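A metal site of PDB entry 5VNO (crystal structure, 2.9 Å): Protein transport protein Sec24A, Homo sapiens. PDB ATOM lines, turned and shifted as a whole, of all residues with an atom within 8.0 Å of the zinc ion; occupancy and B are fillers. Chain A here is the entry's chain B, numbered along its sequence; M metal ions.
The side-chain sulfur of Cys 89 sits close to the side-chain hydroxyl of Thr 91, at 3.0 Å.
O of Cys 89 is in hydrogen-bond range of NE of Arg 407 (3.1 Å).
O of Thr 91 is in hydrogen-bond range of N of Cys 86, 3.0 Å away.
The backbone NH (N) of Ser 88 sits close to the side-chain sulfur (SG) of Cys 86, 3.4 Å away.
The side-chain sulfur (SG) of Cys 86 sits close to the side-chain amide nitrogen (ND2) of Asn 114 (3.2 Å).
SG of Cys 107 lies close to N of Leu 109 (3.5 Å).
N of Cys 107 is in hydrogen-bond range of O of Arg 112 (2.9 Å).
The zinc ion is bound by SG of Cys 89, SG of Cys 86, SG of Cys 110 and SG of Cys 107.
The zinc ion has four donor atoms within binding distance.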
ATOM      1  N   ARG A  85     -15.051  -1.252 -14.085  1.00  0.00           N
ATOM      2  CA  ARG A  85     -14.458  -0.133 -13.367  1.00  0.00           C
ATOM      3  C   ARG A  85     -15.569   0.675 -12.704  1.00  0.00           C
ATOM      4  O   ARG A  85     -16.653   0.826 -13.267  1.00  0.00           O
ATOM      5  CB  ARG A  85     -13.633   0.774 -14.300  1.00  0.00           C
ATOM      6  CG  ARG A  85     -12.477   0.058 -14.993  1.00  0.00           C
ATOM      7  CD  ARG A  85     -11.733   0.986 -15.955  1.00  0.00           C
ATOM      8  NE  ARG A  85     -10.949   2.011 -15.266  1.00  0.00           N
ATOM      9  CZ  ARG A  85     -10.173   2.897 -15.870  1.00  0.00           C
ATOM     10  NH1 ARG A  85     -10.052   2.897 -17.199  1.00  0.00           N
ATOM     11  NH2 ARG A  85      -9.498   3.784 -15.155  1.00  0.00           N
ATOM     12  N   CYS A  86     -15.280   1.195 -11.513  1.00  0.00           N
ATOM     13  CA  CYS A  86     -16.241   2.037 -10.816  1.00  0.00           C
ATOM     14  C   CYS A  86     -16.641   3.223 -11.685  1.00  0.00           C
ATOM     15  O   CYS A  86     -15.778   3.873 -12.283  1.00  0.00           O
ATOM     16  CB  CYS A  86     -15.638   2.512  -9.489  1.00  0.00           C
ATOM     17  SG  CYS A  86     -16.550   3.824  -8.656  1.00  0.00           S
ATOM     18  N   ARG A  87     -17.938   3.503 -11.749  1.00  0.00           N
ATOM     19  CA  ARG A  87     -18.448   4.554 -12.614  1.00  0.00           C
ATOM     20  C   ARG A  87     -18.052   5.961 -12.160  1.00  0.00           C
ATOM     21  O   ARG A  87     -18.265   6.910 -12.913  1.00  0.00           O
ATOM     22  CB  ARG A  87     -19.967   4.477 -12.704  1.00  0.00           C
ATOM     23  CG  ARG A  87     -20.493   3.258 -13.451  1.00  0.00           C
ATOM     24  CD  ARG A  87     -22.006   3.303 -13.571  1.00  0.00           C
ATOM     25  NE  ARG A  87     -22.553   2.173 -14.308  1.00  0.00           N
ATOM     26  CZ  ARG A  87     -23.851   1.983 -14.551  1.00  0.00           C
ATOM     27  NH1 ARG A  87     -24.742   2.865 -14.116  1.00  0.00           N
ATOM     28  NH2 ARG A  87     -24.252   0.921 -15.228  1.00  0.00           N
ATOM     29  N   SER A  88     -17.511   6.117 -10.953  1.00  0.00           N
ATOM     30  CA  SER A  88     -17.138   7.429 -10.422  1.00  0.00           C
ATOM     31  C   SER A  88     -15.638   7.688 -10.547  1.00  0.00           C
ATOM     32  O   SER A  88     -15.224   8.597 -11.266  1.00  0.00           O
ATOM     33  CB  SER A  88     -17.585   7.562  -8.967  1.00  0.00           C
ATOM     34  OG  SER A  88     -18.964   7.873  -8.896  1.00  0.00           O
ATOM     35  N   CYS A  89     -14.817   6.917  -9.826  1.00  0.00           N
ATOM     36  CA  CYS A  89     -13.379   7.130  -9.796  1.00  0.00           C
ATOM     37  C   CYS A  89     -12.615   6.228 -10.764  1.00  0.00           C
ATOM     38  O   CYS A  89     -11.390   6.296 -10.820  1.00  0.00           O
ATOM     39  CB  CYS A  89     -12.856   6.908  -8.377  1.00  0.00           C
ATOM     40  SG  CYS A  89     -13.059   5.236  -7.757  1.00  0.00           S
ATOM     41  N   ARG A  90     -13.319   5.392 -11.528  1.00  0.00           N
ATOM     42  CA  ARG A  90     -12.712   4.541 -12.553  1.00  0.00           C
ATOM     43  C   ARG A  90     -11.703   3.550 -11.981  1.00  0.00           C
ATOM     44  O   ARG A  90     -10.888   2.999 -12.724  1.00  0.00           O
ATOM     45  CB  ARG A  90     -12.049   5.373 -13.650  1.00  0.00           C
ATOM     46  CG  ARG A  90     -12.969   6.393 -14.314  1.00  0.00           C
ATOM     47  CD  ARG A  90     -14.326   5.793 -14.689  1.00  0.00           C
ATOM     48  NE  ARG A  90     -14.206   4.564 -15.464  1.00  0.00           N
ATOM     49  CZ  ARG A  90     -14.136   4.500 -16.786  1.00  0.00           C
ATOM     50  NH1 ARG A  90     -14.161   5.599 -17.522  1.00  0.00           N
ATOM     51  NH2 ARG A  90     -14.023   3.318 -17.391  1.00  0.00           N
ATOM     52  N   THR A  91     -11.759   3.293 -10.679  1.00  0.00           N
ATOM     53  CA  THR A  91     -10.892   2.284 -10.089  1.00  0.00           C
ATOM     54  C   THR A  91     -11.299   0.907 -10.574  1.00  0.00           C
ATOM     55  O   THR A  91     -12.490   0.583 -10.637  1.00  0.00           O
ATOM     56  CB  THR A  91     -10.955   2.341  -8.564  1.00  0.00           C
ATOM     57  OG1 THR A  91     -10.538   3.635  -8.104  1.00  0.00           O
ATOM     58  CG2 THR A  91     -10.057   1.279  -7.939  1.00  0.00           C
ATOM     59  N   TYR A  92     -10.310   0.081 -10.900  1.00  0.00           N
ATOM     60  CA  TYR A  92     -10.594  -1.255 -11.407  1.00  0.00           C
ATOM     61  C   TYR A  92     -11.083  -2.166 -10.299  1.00  0.00           C
ATOM     62  O   TYR A  92     -10.699  -2.029  -9.127  1.00  0.00           O
ATOM     63  CB  TYR A  92      -9.352  -1.838 -12.065  1.00  0.00           C
ATOM     64  CG  TYR A  92      -8.864  -1.076 -13.278  1.00  0.00           C
ATOM     65  CD1 TYR A  92      -8.083   0.069 -13.146  1.00  0.00           C
ATOM     66  CD2 TYR A  92      -9.181  -1.497 -14.563  1.00  0.00           C
ATOM     67  CE1 TYR A  92      -7.648   0.770 -14.252  1.00  0.00           C
ATOM     68  CE2 TYR A  92      -8.743  -0.808 -15.675  1.00  0.00           C
ATOM     69  CZ  TYR A  92      -7.971   0.329 -15.516  1.00  0.00           C
ATOM     70  OH  TYR A  92      -7.531   1.027 -16.614  1.00  0.00           O
ATOM     71  N   ASN A  94     -11.200  -4.847  -7.814  1.00  0.00           N
ATOM     72  CA  ASN A  94     -10.052  -5.412  -7.103  1.00  0.00           C
ATOM     73  C   ASN A  94     -10.531  -6.381  -6.035  1.00  0.00           C
ATOM     74  O   ASN A  94     -11.713  -6.414  -5.685  1.00  0.00           O
ATOM     75  CB  ASN A  94      -9.218  -4.296  -6.472  1.00  0.00           C
ATOM     76  CG  ASN A  94      -9.980  -3.514  -5.415  1.00  0.00           C
ATOM     77  OD1 ASN A  94      -9.928  -3.839  -4.229  1.00  0.00           O
ATOM     78  ND2 ASN A  94     -10.699  -2.490  -5.843  1.00  0.00           N
ATOM     79  N   TRP A 105     -21.504  -4.079  -6.160  1.00  0.00           N
ATOM     80  CA  TRP A 105     -20.255  -4.059  -5.399  1.00  0.00           C
ATOM     81  C   TRP A 105     -19.915  -2.630  -5.013  1.00  0.00           C
ATOM     82  O   TRP A 105     -20.121  -1.694  -5.800  1.00  0.00           O
ATOM     83  CB  TRP A 105     -19.112  -4.682  -6.197  1.00  0.00           C
ATOM     84  CG  TRP A 105     -18.755  -3.941  -7.461  1.00  0.00           C
ATOM     85  CD1 TRP A 105     -19.418  -4.001  -8.656  1.00  0.00           C
ATOM     86  CD2 TRP A 105     -17.652  -3.047  -7.669  1.00  0.00           C
ATOM     87  NE1 TRP A 105     -18.798  -3.205  -9.580  1.00  0.00           N
ATOM     88  CE2 TRP A 105     -17.713  -2.605  -9.003  1.00  0.00           C
ATOM     89  CE3 TRP A 105     -16.622  -2.572  -6.848  1.00  0.00           C
ATOM     90  CZ2 TRP A 105     -16.785  -1.712  -9.536  1.00  0.00           C
ATOM     91  CZ3 TRP A 105     -15.710  -1.693  -7.376  1.00  0.00           C
ATOM     92  CH2 TRP A 105     -15.787  -1.266  -8.706  1.00  0.00           C
ATOM     93  N   LYS A 106     -19.413  -2.467  -3.791  1.00  0.00           N
ATOM     94  CA  LYS A 106     -19.019  -1.153  -3.286  1.00  0.00           C
ATOM     95  C   LYS A 106     -17.540  -0.937  -3.586  1.00  0.00           C
ATOM     96  O   LYS A 106     -16.691  -1.743  -3.204  1.00  0.00           O
ATOM     97  CB  LYS A 106     -19.285  -1.059  -1.783  1.00  0.00           C
ATOM     98  CG  LYS A 106     -18.706   0.196  -1.128  1.00  0.00           C
ATOM     99  CD  LYS A 106     -19.056   0.278   0.359  1.00  0.00           C
ATOM    100  CE  LYS A 106     -20.545   0.478   0.578  1.00  0.00           C
ATOM    101  NZ  LYS A 106     -20.892   0.595   2.016  1.00  0.00           N
ATOM    102  N   CYS A 107     -17.248   0.167  -4.280  1.00  0.00           N
ATOM    103  CA  CYS A 107     -15.860   0.516  -4.549  1.00  0.00           C
ATOM    104  C   CYS A 107     -15.145   0.824  -3.242  1.00  0.00           C
ATOM    105  O   CYS A 107     -15.668   1.520  -2.364  1.00  0.00           O
ATOM    106  CB  CYS A 107     -15.808   1.725  -5.474  1.00  0.00           C
ATOM    107  SG  CYS A 107     -14.143   2.222  -5.991  1.00  0.00           S
ATOM    108  N   ASN A 108     -13.934   0.289  -3.087  1.00  0.00           N
ATOM    109  CA  ASN A 108     -13.129   0.480  -1.891  1.00  0.00           C
ATOM    110  C   ASN A 108     -12.252   1.725  -1.952  1.00  0.00           C
ATOM    111  O   ASN A 108     -11.375   1.883  -1.109  1.00  0.00           O
ATOM    112  CB  ASN A 108     -12.260  -0.754  -1.635  1.00  0.00           C
ATOM    113  CG  ASN A 108     -11.395  -1.119  -2.817  1.00  0.00           C
ATOM    114  OD1 ASN A 108     -11.754  -0.855  -3.963  1.00  0.00           O
ATOM    115  ND2 ASN A 108     -10.252  -1.729  -2.551  1.00  0.00           N
ATOM    116  N   LEU A 109     -12.471   2.593  -2.941  1.00  0.00           N
ATOM    117  CA  LEU A 109     -11.700   3.828  -3.063  1.00  0.00           C
ATOM    118  C   LEU A 109     -12.569   5.084  -3.005  1.00  0.00           C
ATOM    119  O   LEU A 109     -12.148   6.088  -2.424  1.00  0.00           O
ATOM    120  CB  LEU A 109     -10.873   3.829  -4.367  1.00  0.00           C
ATOM    121  CG  LEU A 109      -9.484   3.172  -4.243  1.00  0.00           C
ATOM    122  CD1 LEU A 109      -9.570   1.656  -4.116  1.00  0.00           C
ATOM    123  CD2 LEU A 109      -8.607   3.564  -5.416  1.00  0.00           C
ATOM    124  N   CYS A 110     -13.777   5.053  -3.586  1.00  0.00           N
ATOM    125  CA  CYS A 110     -14.701   6.179  -3.506  1.00  0.00           C
ATOM    126  C   CYS A 110     -16.050   5.787  -2.920  1.00  0.00           C
ATOM    127  O   CYS A 110     -16.963   6.616  -2.861  1.00  0.00           O
ATOM    128  CB  CYS A 110     -14.891   6.835  -4.888  1.00  0.00           C
ATOM    129  SG  CYS A 110     -15.904   5.942  -6.101  1.00  0.00           S
ATOM    130  N   TYR A 111     -16.195   4.536  -2.470  1.00  0.00           N
ATOM    131  CA  TYR A 111     -17.350   4.079  -1.720  1.00  0.00           C
ATOM    132  C   TYR A 111     -18.641   4.072  -2.525  1.00  0.00           C
ATOM    133  O   TYR A 111     -19.708   3.821  -1.971  1.00  0.00           O
ATOM    134  CB  TYR A 111     -17.549   4.919  -0.442  1.00  0.00           C
ATOM    135  CG  TYR A 111     -16.311   5.016   0.417  1.00  0.00           C
ATOM    136  CD1 TYR A 111     -15.459   3.932   0.582  1.00  0.00           C
ATOM    137  CD2 TYR A 111     -15.996   6.202   1.083  1.00  0.00           C
ATOM    138  CE1 TYR A 111     -14.324   4.020   1.364  1.00  0.00           C
ATOM    139  CE2 TYR A 111     -14.869   6.293   1.872  1.00  0.00           C
ATOM    140  CZ  TYR A 111     -14.037   5.209   2.011  1.00  0.00           C
ATOM    141  OH  TYR A 111     -12.914   5.303   2.792  1.00  0.00           O
ATOM    142  N   ARG A 112     -18.576   4.347  -3.826  1.00  0.00           N
ATOM    143  CA  ARG A 112     -19.773   4.294  -4.656  1.00  0.00           C
ATOM    144  C   ARG A 112     -20.154   2.844  -4.927  1.00  0.00           C
ATOM    145  O   ARG A 112     -19.292   1.982  -5.102  1.00  0.00           O
ATOM    146  CB  ARG A 112     -19.562   5.046  -5.976  1.00  0.00           C
ATOM    147  CG  ARG A 112     -20.317   4.460  -7.192  1.00  0.00           C
ATOM    148  CD  ARG A 112     -20.966   5.513  -8.045  1.00  0.00           C
ATOM    149  NE  ARG A 112     -21.859   4.890  -9.019  1.00  0.00           N
ATOM    150  CZ  ARG A 112     -22.445   5.529 -10.019  1.00  0.00           C
ATOM    151  NH1 ARG A 112     -22.247   6.823 -10.202  1.00  0.00           N
ATOM    152  NH2 ARG A 112     -23.225   4.861 -10.857  1.00  0.00           N
ATOM    153  N   VAL A 113     -21.454   2.582  -4.924  1.00  0.00           N
ATOM    154  CA  VAL A 113     -21.988   1.271  -5.283  1.00  0.00           C
ATOM    155  C   VAL A 113     -22.094   1.187  -6.801  1.00  0.00           C
ATOM    156  O   VAL A 113     -22.629   2.100  -7.445  1.00  0.00           O
ATOM    157  CB  VAL A 113     -23.355   1.041  -4.624  1.00  0.00           C
ATOM    158  CG1 VAL A 113     -23.809  -0.400  -4.822  1.00  0.00           C
ATOM    159  CG2 VAL A 113     -23.305   1.380  -3.135  1.00  0.00           C
ATOM    160  N   ASN A 114     -21.587   0.094  -7.366  1.00  0.00           N
ATOM    161  CA  ASN A 114     -21.639  -0.124  -8.808  1.00  0.00           C
ATOM    162  C   ASN A 114     -22.363  -1.421  -9.107  1.00  0.00           C
ATOM    163  O   ASN A 114     -22.418  -2.329  -8.274  1.00  0.00           O
ATOM    164  CB  ASN A 114     -20.230  -0.166  -9.411  1.00  0.00           C
ATOM    165  CG  ASN A 114     -19.590   1.202  -9.502  1.00  0.00           C
ATOM    166  OD1 ASN A 114     -19.712   1.888 -10.520  1.00  0.00           O
ATOM    167  ND2 ASN A 114     -18.898   1.607  -8.452  1.00  0.00           N
ATOM    168  N   ARG A 407      -4.112   5.499  -7.761  1.00  0.00           N
ATOM    169  CA  ARG A 407      -5.344   5.849  -7.074  1.00  0.00           C
ATOM    170  C   ARG A 407      -5.278   5.397  -5.625  1.00  0.00           C
ATOM    171  O   ARG A 407      -4.743   4.329  -5.323  1.00  0.00           O
ATOM    172  CB  ARG A 407      -6.551   5.219  -7.774  1.00  0.00           C
ATOM    173  CG  ARG A 407      -6.782   5.741  -9.182  1.00  0.00           C
ATOM    174  CD  ARG A 407      -8.013   5.107  -9.807  1.00  0.00           C
ATOM    175  NE  ARG A 407      -8.326   5.675 -11.123  1.00  0.00           N
ATOM    176  CZ  ARG A 407      -7.882   5.208 -12.286  1.00  0.00           C
ATOM    177  NH1 ARG A 407      -7.091   4.135 -12.326  1.00  0.00           N
ATOM    178  NH2 ARG A 407      -8.226   5.800 -13.414  1.00  0.00           N
HETATM  179 ZN    ZN M   1     -14.907   4.132  -7.176  1.00  0.00          ZN
